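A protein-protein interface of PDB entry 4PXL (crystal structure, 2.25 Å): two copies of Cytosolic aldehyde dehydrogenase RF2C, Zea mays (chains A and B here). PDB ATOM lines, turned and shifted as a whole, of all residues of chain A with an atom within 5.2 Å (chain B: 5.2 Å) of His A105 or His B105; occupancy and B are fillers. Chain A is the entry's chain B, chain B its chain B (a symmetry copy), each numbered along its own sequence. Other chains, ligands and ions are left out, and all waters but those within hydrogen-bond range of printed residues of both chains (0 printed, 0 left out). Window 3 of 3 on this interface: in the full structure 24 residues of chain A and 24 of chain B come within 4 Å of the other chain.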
ATOM      1  N   ARG A 100      -6.786  35.731 -19.489  1.00  0.00           N
ATOM      2  CA  ARG A 100      -5.932  34.958 -20.405  1.00  0.00           C
ATOM      3  C   ARG A 100      -6.538  33.545 -20.526  1.00  0.00           C
ATOM      4  O   ARG A 100      -6.642  33.030 -21.635  1.00  0.00           O
ATOM      5  CB  ARG A 100      -4.474  34.889 -19.920  1.00  0.00           C
ATOM      6  CG  ARG A 100      -3.642  36.145 -20.237  1.00  0.00           C
ATOM      7  CD  ARG A 100      -2.176  35.916 -19.940  1.00  0.00           C
ATOM      8  NE  ARG A 100      -1.936  35.666 -18.514  1.00  0.00           N
ATOM      9  CZ  ARG A 100      -1.732  36.622 -17.617  1.00  0.00           C
ATOM     10  NH1 ARG A 100      -1.698  37.895 -17.991  1.00  0.00           N
ATOM     11  NH2 ARG A 100      -1.549  36.316 -16.340  1.00  0.00           N
ATOM     12  N   GLY A 101      -7.024  32.996 -19.398  1.00  0.00           N
ATOM     13  CA  GLY A 101      -7.694  31.699 -19.319  1.00  0.00           C
ATOM     14  C   GLY A 101      -8.945  31.637 -20.173  1.00  0.00           C
ATOM     15  O   GLY A 101      -9.169  30.648 -20.864  1.00  0.00           O
ATOM     16  N   ARG A 102      -9.752  32.686 -20.158  1.00  0.00           N
ATOM     17  CA  ARG A 102     -10.985  32.728 -20.950  1.00  0.00           C
ATOM     18  C   ARG A 102     -10.658  32.675 -22.442  1.00  0.00           C
ATOM     19  O   ARG A 102     -11.330  31.969 -23.198  1.00  0.00           O
ATOM     20  CB  ARG A 102     -11.829  33.974 -20.615  1.00  0.00           C
ATOM     21  CG  ARG A 102     -12.383  33.997 -19.187  1.00  0.00           C
ATOM     22  CD  ARG A 102     -13.738  33.360 -19.126  1.00  0.00           C
ATOM     23  NE  ARG A 102     -14.802  34.342 -19.313  1.00  0.00           N
ATOM     24  CZ  ARG A 102     -16.018  34.031 -19.746  1.00  0.00           C
ATOM     25  NH1 ARG A 102     -16.940  34.974 -19.881  1.00  0.00           N
ATOM     26  NH2 ARG A 102     -16.322  32.772 -20.049  1.00  0.00           N
ATOM     27  N   ILE A 103      -9.600  33.408 -22.849  1.00  0.00           N
ATOM     28  CA  ILE A 103      -9.112  33.411 -24.217  1.00  0.00           C
ATOM     29  C   ILE A 103      -8.583  31.999 -24.592  1.00  0.00           C
ATOM     30  O   ILE A 103      -8.898  31.517 -25.671  1.00  0.00           O
ATOM     31  CB  ILE A 103      -8.098  34.562 -24.461  1.00  0.00           C
ATOM     32  CG1 ILE A 103      -8.819  35.909 -24.560  1.00  0.00           C
ATOM     33  CG2 ILE A 103      -7.250  34.310 -25.726  1.00  0.00           C
ATOM     34  CD1 ILE A 103      -7.915  37.126 -24.273  1.00  0.00           C
ATOM     35  N   LEU A 104      -7.846  31.323 -23.686  1.00  0.00           N
ATOM     36  CA  LEU A 104      -7.335  29.986 -23.946  1.00  0.00           C
ATOM     37  C   LEU A 104      -8.438  28.935 -24.002  1.00  0.00           C
ATOM     38  O   LEU A 104      -8.294  27.958 -24.730  1.00  0.00           O
ATOM     39  CB  LEU A 104      -6.215  29.583 -22.967  1.00  0.00           C
ATOM     40  CG  LEU A 104      -4.971  30.452 -22.941  1.00  0.00           C
ATOM     41  CD1 LEU A 104      -3.979  29.913 -21.951  1.00  0.00           C
ATOM     42  CD2 LEU A 104      -4.337  30.611 -24.315  1.00  0.00           C
ATOM     43  N   HIS A 105      -9.524  29.124 -23.230  1.00  0.00           N
ATOM     44  CA  HIS A 105     -10.674  28.224 -23.239  1.00  0.00           C
ATOM     45  C   HIS A 105     -11.414  28.311 -24.595  1.00  0.00           C
ATOM     46  O   HIS A 105     -11.914  27.299 -25.079  1.00  0.00           O
ATOM     47  CB  HIS A 105     -11.649  28.527 -22.090  1.00  0.00           C
ATOM     48  CG  HIS A 105     -11.348  27.765 -20.835  1.00  0.00           C
ATOM     49  ND1 HIS A 105     -10.985  28.446 -19.674  1.00  0.00           N
ATOM     50  CD2 HIS A 105     -11.315  26.439 -20.575  1.00  0.00           C
ATOM     51  CE1 HIS A 105     -10.745  27.525 -18.757  1.00  0.00           C
ATOM     52  NE2 HIS A 105     -10.916  26.310 -19.240  1.00  0.00           N
ATOM     53  N   ARG A 106     -11.505  29.528 -25.170  1.00  0.00           N
ATOM     54  CA  ARG A 106     -12.078  29.780 -26.488  1.00  0.00           C
ATOM     55  C   ARG A 106     -11.183  29.156 -27.580  1.00  0.00           C
ATOM     56  O   ARG A 106     -11.687  28.566 -28.523  1.00  0.00           O
ATOM     57  CB  ARG A 106     -12.313  31.297 -26.696  1.00  0.00           C
ATOM     58  CG  ARG A 106     -12.927  31.707 -28.062  1.00  0.00           C
ATOM     59  CD  ARG A 106     -14.154  30.900 -28.474  1.00  0.00           C
ATOM     60  NE  ARG A 106     -14.718  31.332 -29.756  1.00  0.00           N
ATOM     61  CZ  ARG A 106     -15.708  30.703 -30.383  1.00  0.00           C
ATOM     62  NH1 ARG A 106     -16.166  31.162 -31.542  1.00  0.00           N
ATOM     63  NH2 ARG A 106     -16.244  29.605 -29.861  1.00  0.00           N
ATOM     64  N   PHE A 107      -9.865  29.237 -27.405  1.00  0.00           N
ATOM     65  CA  PHE A 107      -8.878  28.661 -28.290  1.00  0.00           C
ATOM     66  C   PHE A 107      -9.048  27.125 -28.301  1.00  0.00           C
ATOM     67  O   PHE A 107      -9.115  26.545 -29.393  1.00  0.00           O
ATOM     68  CB  PHE A 107      -7.460  29.140 -27.883  1.00  0.00           C
ATOM     69  CG  PHE A 107      -6.272  28.780 -28.762  1.00  0.00           C
ATOM     70  CD1 PHE A 107      -6.451  28.113 -29.971  1.00  0.00           C
ATOM     71  CD2 PHE A 107      -4.976  29.071 -28.355  1.00  0.00           C
ATOM     72  CE1 PHE A 107      -5.355  27.750 -30.758  1.00  0.00           C
ATOM     73  CE2 PHE A 107      -3.883  28.709 -29.144  1.00  0.00           C
ATOM     74  CZ  PHE A 107      -4.079  28.051 -30.343  1.00  0.00           C
ATOM     75  N   ALA A 108      -9.200  26.497 -27.106  1.00  0.00           N
ATOM     76  CA  ALA A 108      -9.430  25.052 -26.961  1.00  0.00           C
ATOM     77  C   ALA A 108     -10.747  24.642 -27.653  1.00  0.00           C
ATOM     78  O   ALA A 108     -10.774  23.632 -28.358  1.00  0.00           O
ATOM     79  CB  ALA A 108      -9.469  24.668 -25.495  1.00  0.00           C
ATOM     80  N   ASP A 109     -11.824  25.432 -27.474  1.00  0.00           N
ATOM     81  CA  ASP A 109     -13.101  25.145 -28.138  1.00  0.00           C
ATOM     82  C   ASP A 109     -12.965  25.140 -29.661  1.00  0.00           C
ATOM     83  O   ASP A 109     -13.510  24.253 -30.307  1.00  0.00           O
ATOM     84  CB  ASP A 109     -14.210  26.107 -27.688  1.00  0.00           C
ATOM     85  CG  ASP A 109     -14.643  25.955 -26.239  1.00  0.00           C
ATOM     86  OD1 ASP A 109     -14.557  24.827 -25.706  1.00  0.00           O
ATOM     87  OD2 ASP A 109     -15.093  26.958 -25.649  1.00  0.00           O
ATOM     88  N   ARG A 146      -7.008  23.498 -21.939  1.00  0.00           N
ATOM     89  CA  ARG A 146      -8.031  23.757 -20.904  1.00  0.00           C
ATOM     90  C   ARG A 146      -7.421  23.625 -19.521  1.00  0.00           C
ATOM     91  O   ARG A 146      -7.765  24.391 -18.618  1.00  0.00           O
ATOM     92  CB  ARG A 146      -9.220  22.790 -21.015  1.00  0.00           C
ATOM     93  CG  ARG A 146     -10.118  23.130 -22.152  1.00  0.00           C
ATOM     94  CD  ARG A 146     -11.329  22.240 -22.214  1.00  0.00           C
ATOM     95  NE  ARG A 146     -12.118  22.638 -23.367  1.00  0.00           N
ATOM     96  CZ  ARG A 146     -12.169  21.960 -24.491  1.00  0.00           C
ATOM     97  NH1 ARG A 146     -12.874  22.422 -25.515  1.00  0.00           N
ATOM     98  NH2 ARG A 146     -11.547  20.795 -24.596  1.00  0.00           N
ATOM     99  N   ALA A 149      -5.494  26.867 -19.100  1.00  0.00           N
ATOM    100  CA  ALA A 149      -6.462  27.953 -19.007  1.00  0.00           C
ATOM    101  C   ALA A 149      -7.019  27.990 -17.556  1.00  0.00           C
ATOM    102  O   ALA A 149      -7.097  29.068 -16.951  1.00  0.00           O
ATOM    103  CB  ALA A 149      -7.589  27.736 -20.003  1.00  0.00           C
ATOM    104  N   GLY A 150      -7.303  26.811 -16.990  1.00  0.00           N
ATOM    105  CA  GLY A 150      -7.810  26.694 -15.624  1.00  0.00           C
ATOM    106  C   GLY A 150      -6.775  26.999 -14.556  1.00  0.00           C
ATOM    107  O   GLY A 150      -7.147  27.267 -13.415  1.00  0.00           O
ATOM    108  N   ARG B 100     -16.011  16.862 -14.299  1.00  0.00           N
ATOM    109  CA  ARG B 100     -16.861  17.635 -13.378  1.00  0.00           C
ATOM    110  C   ARG B 100     -16.678  19.128 -13.718  1.00  0.00           C
ATOM    111  O   ARG B 100     -17.666  19.850 -13.798  1.00  0.00           O
ATOM    112  CB  ARG B 100     -16.517  17.362 -11.905  1.00  0.00           C
ATOM    113  CG  ARG B 100     -17.124  16.064 -11.343  1.00  0.00           C
ATOM    114  CD  ARG B 100     -16.939  15.979  -9.844  1.00  0.00           C
ATOM    115  NE  ARG B 100     -15.522  15.914  -9.468  1.00  0.00           N
ATOM    116  CZ  ARG B 100     -14.827  14.788  -9.386  1.00  0.00           C
ATOM    117  NH1 ARG B 100     -15.414  13.620  -9.614  1.00  0.00           N
ATOM    118  NH2 ARG B 100     -13.540  14.815  -9.065  1.00  0.00           N
ATOM    119  N   GLY B 101     -15.430  19.532 -14.018  1.00  0.00           N
ATOM    120  CA  GLY B 101     -15.065  20.887 -14.428  1.00  0.00           C
ATOM    121  C   GLY B 101     -15.767  21.320 -15.700  1.00  0.00           C
ATOM    122  O   GLY B 101     -16.253  22.443 -15.781  1.00  0.00           O
ATOM    123  N   ARG B 102     -15.852  20.440 -16.684  1.00  0.00           N
ATOM    124  CA  ARG B 102     -16.515  20.757 -17.954  1.00  0.00           C
ATOM    125  C   ARG B 102     -18.001  21.031 -17.722  1.00  0.00           C
ATOM    126  O   ARG B 102     -18.554  21.969 -18.300  1.00  0.00           O
ATOM    127  CB  ARG B 102     -16.316  19.634 -18.990  1.00  0.00           C
ATOM    128  CG  ARG B 102     -14.866  19.441 -19.443  1.00  0.00           C
ATOM    129  CD  ARG B 102     -14.563  20.277 -20.650  1.00  0.00           C
ATOM    130  NE  ARG B 102     -14.809  19.544 -21.888  1.00  0.00           N
ATOM    131  CZ  ARG B 102     -15.060  20.133 -23.050  1.00  0.00           C
ATOM    132  NH1 ARG B 102     -15.263  19.403 -24.138  1.00  0.00           N
ATOM    133  NH2 ARG B 102     -15.112  21.459 -23.134  1.00  0.00           N
ATOM    134  N   ILE B 103     -18.629  20.216 -16.848  1.00  0.00           N
ATOM    135  CA  ILE B 103     -20.019  20.384 -16.462  1.00  0.00           C
ATOM    136  C   ILE B 103     -20.198  21.729 -15.705  1.00  0.00           C
ATOM    137  O   ILE B 103     -21.142  22.451 -15.996  1.00  0.00           O
ATOM    138  CB  ILE B 103     -20.555  19.142 -15.697  1.00  0.00           C
ATOM    139  CG1 ILE B 103     -20.811  17.981 -16.661  1.00  0.00           C
ATOM    140  CG2 ILE B 103     -21.836  19.476 -14.903  1.00  0.00           C
ATOM    141  CD1 ILE B 103     -20.827  16.595 -15.982  1.00  0.00           C
ATOM    142  N   LEU B 104     -19.266  22.089 -14.796  1.00  0.00           N
ATOM    143  CA  LEU B 104     -19.343  23.344 -14.064  1.00  0.00           C
ATOM    144  C   LEU B 104     -19.110  24.560 -14.954  1.00  0.00           C
ATOM    145  O   LEU B 104     -19.670  25.616 -14.680  1.00  0.00           O
ATOM    146  CB  LEU B 104     -18.425  23.360 -12.826  1.00  0.00           C
ATOM    147  CG  LEU B 104     -18.670  22.302 -11.766  1.00  0.00           C
ATOM    148  CD1 LEU B 104     -17.706  22.470 -10.628  1.00  0.00           C
ATOM    149  CD2 LEU B 104     -20.108  22.295 -11.266  1.00  0.00           C
ATOM    150  N   HIS B 105     -18.278  24.419 -16.002  1.00  0.00           N
ATOM    151  CA  HIS B 105     -18.019  25.488 -16.963  1.00  0.00           C
ATOM    152  C   HIS B 105     -19.290  25.782 -17.795  1.00  0.00           C
ATOM    153  O   HIS B 105     -19.543  26.937 -18.128  1.00  0.00           O
ATOM    154  CB  HIS B 105     -16.848  25.148 -17.899  1.00  0.00           C
ATOM    155  CG  HIS B 105     -15.518  25.601 -17.379  1.00  0.00           C
ATOM    156  ND1 HIS B 105     -14.532  24.663 -17.073  1.00  0.00           N
ATOM    157  CD2 HIS B 105     -15.039  26.829 -17.083  1.00  0.00           C
ATOM    158  CE1 HIS B 105     -13.499  25.343 -16.606  1.00  0.00           C
ATOM    159  NE2 HIS B 105     -13.748  26.637 -16.580  1.00  0.00           N
ATOM    160  N   ARG B 106     -20.054  24.727 -18.148  1.00  0.00           N
ATOM    161  CA  ARG B 106     -21.332  24.826 -18.844  1.00  0.00           C
ATOM    162  C   ARG B 106     -22.384  25.480 -17.923  1.00  0.00           C
ATOM    163  O   ARG B 106     -23.158  26.313 -18.370  1.00  0.00           O
ATOM    164  CB  ARG B 106     -21.772  23.437 -19.370  1.00  0.00           C
ATOM    165  CG  ARG B 106     -23.120  23.399 -20.139  1.00  0.00           C
ATOM    166  CD  ARG B 106     -23.265  24.466 -21.219  1.00  0.00           C
ATOM    167  NE  ARG B 106     -24.540  24.384 -21.938  1.00  0.00           N
ATOM    168  CZ  ARG B 106     -24.949  25.278 -22.832  1.00  0.00           C
ATOM    169  NH1 ARG B 106     -26.119  25.128 -23.443  1.00  0.00           N
ATOM    170  NH2 ARG B 106     -24.197  26.335 -23.120  1.00  0.00           N
ATOM    171  N   PHE B 107     -22.356  25.144 -16.635  1.00  0.00           N
ATOM    172  CA  PHE B 107     -23.223  25.697 -15.619  1.00  0.00           C
ATOM    173  C   PHE B 107     -22.955  27.215 -15.501  1.00  0.00           C
ATOM    174  O   PHE B 107     -23.919  27.990 -15.531  1.00  0.00           O
ATOM    175  CB  PHE B 107     -23.045  24.915 -14.291  1.00  0.00           C
ATOM    176  CG  PHE B 107     -23.964  25.224 -13.118  1.00  0.00           C
ATOM    177  CD1 PHE B 107     -25.016  26.125 -13.249  1.00  0.00           C
ATOM    178  CD2 PHE B 107     -23.742  24.645 -11.873  1.00  0.00           C
ATOM    179  CE1 PHE B 107     -25.835  26.435 -12.159  1.00  0.00           C
ATOM    180  CE2 PHE B 107     -24.561  24.956 -10.787  1.00  0.00           C
ATOM    181  CZ  PHE B 107     -25.605  25.849 -10.937  1.00  0.00           C
ATOM    182  N   ALA B 108     -21.660  27.626 -15.453  1.00  0.00           N
ATOM    183  CA  ALA B 108     -21.249  29.036 -15.401  1.00  0.00           C
ATOM    184  C   ALA B 108     -21.727  29.787 -16.662  1.00  0.00           C
ATOM    185  O   ALA B 108     -22.242  30.900 -16.547  1.00  0.00           O
ATOM    186  CB  ALA B 108     -19.742  29.142 -15.271  1.00  0.00           C
ATOM    187  N   ASP B 109     -21.580  29.174 -17.852  1.00  0.00           N
ATOM    188  CA  ASP B 109     -22.056  29.793 -19.094  1.00  0.00           C
ATOM    189  C   ASP B 109     -23.561  30.057 -19.061  1.00  0.00           C
ATOM    190  O   ASP B 109     -23.990  31.129 -19.473  1.00  0.00           O
ATOM    191  CB  ASP B 109     -21.670  28.968 -20.331  1.00  0.00           C
ATOM    192  CG  ASP B 109     -20.181  28.920 -20.631  1.00  0.00           C
ATOM    193  OD1 ASP B 109     -19.474  29.897 -20.302  1.00  0.00           O
ATOM    194  OD2 ASP B 109     -19.729  27.917 -21.220  1.00  0.00           O
ATOM    195  N   ARG B 146     -16.299  29.192 -12.404  1.00  0.00           N
ATOM    196  CA  ARG B 146     -15.227  28.924 -13.387  1.00  0.00           C
ATOM    197  C   ARG B 146     -13.909  28.691 -12.672  1.00  0.00           C
ATOM    198  O   ARG B 146     -13.121  27.840 -13.092  1.00  0.00           O
ATOM    199  CB  ARG B 146     -15.054  30.084 -14.379  1.00  0.00           C
ATOM    200  CG  ARG B 146     -16.137  30.120 -15.398  1.00  0.00           C
ATOM    201  CD  ARG B 146     -15.926  31.200 -16.424  1.00  0.00           C
ATOM    202  NE  ARG B 146     -17.047  31.163 -17.348  1.00  0.00           N
ATOM    203  CZ  ARG B 146     -18.028  32.038 -17.347  1.00  0.00           C
ATOM    204  NH1 ARG B 146     -19.042  31.901 -18.192  1.00  0.00           N
ATOM    205  NH2 ARG B 146     -17.993  33.077 -16.528  1.00  0.00           N
ATOM    206  N   ALA B 149     -14.241  25.145 -11.358  1.00  0.00           N
ATOM    207  CA  ALA B 149     -14.240  24.244 -12.503  1.00  0.00           C
ATOM    208  C   ALA B 149     -12.769  24.032 -12.960  1.00  0.00           C
ATOM    209  O   ALA B 149     -12.352  22.891 -13.197  1.00  0.00           O
ATOM    210  CB  ALA B 149     -15.068  24.831 -13.634  1.00  0.00           C
ATOM    211  N   GLY B 150     -11.984  25.116 -12.981  1.00  0.00           N
ATOM    212  CA  GLY B 150     -10.575  25.062 -13.366  1.00  0.00           C
ATOM    213  C   GLY B 150      -9.682  24.392 -12.337  1.00  0.00           C
ATOM    214  O   GLY B 150      -8.573  23.984 -12.676  1.00  0.00           O
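NH2 of Arg B102 sits close to NE of Arg A146, at 3.2 Å.
NH2 of Arg A102 sits close to NE of Arg B146.
Arg A102 touches Arg B146, and with the chains exchanged Arg A146 touches Arg B102.
His A105 touches its own counterpart, His B105.
Gly B150 touches its own counterpart, Gly A150.
Positions printed for both chains: 100, 101, 102, 103, 104, 105, 106, 107, 108, 109, 146, 149 and 150.
Of the 4 pairs that touch across the chains among the printed residues, 4 have their exchanged pair printed and touching as well.
Hydrophobic or aromatic side chains of chain A within 4 Å of the printed part of chain B: His A105.
Hydrophobic or aromatic side chains of chain B that line the printed part of chain A: His B105.
Among the printed residues, 4 pairs touch across the chains.
The side-chain carboxylate (OD1) of Asp B109 lies within salt-bridge range of the guanidinium group (NH1) of Arg B146, at 2.9 Å.
The backbone carbonyl oxygen (O) of Gly B101 is in hydrogen-bond range of a ring nitrogen (ND1) of His B105, 3.1 Å away.
ND1 of His A105 lies within hydrogen-bond range of O of Gly A101, 3.1 Å away.
OD1 of Asp A109 is in salt-bridge range of NH1 of Arg A146, at 2.9 Å.
Among the printed residues, merely in contact across the chains: Gly A150 with Gly B150 and His A105 with His B105.
Of the printed residues of chain B, Arg A102 touches Arg B146.
His A105 touches just one residue of chain B: His B105.
Asp A109 touches none of the printed residues of chain B.
Of the printed residues of chain B, Arg A146 touches Arg B102 (3.2 Å).
Printed residues of chain B within 4 Å of Gly A150: Gly B150 (3.7 Å).
Gly B101 touches none of the printed residues of chain A.
His B105 touches just one residue of chain A: His A105 (3.8 Å).
Printed residues of chain A within 4 Å of Arg B146: Arg A102 (3.2 Å).
Printed residues of chain A within 4 Å of Gly B150: Gly A150.
The nearest printed residue of chain B that does not touch His A105 is Gly B150 (5.9 Å).
The nearest printed residue of chain A that does not touch Arg B102 is Asp A109 (4.3 Å).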
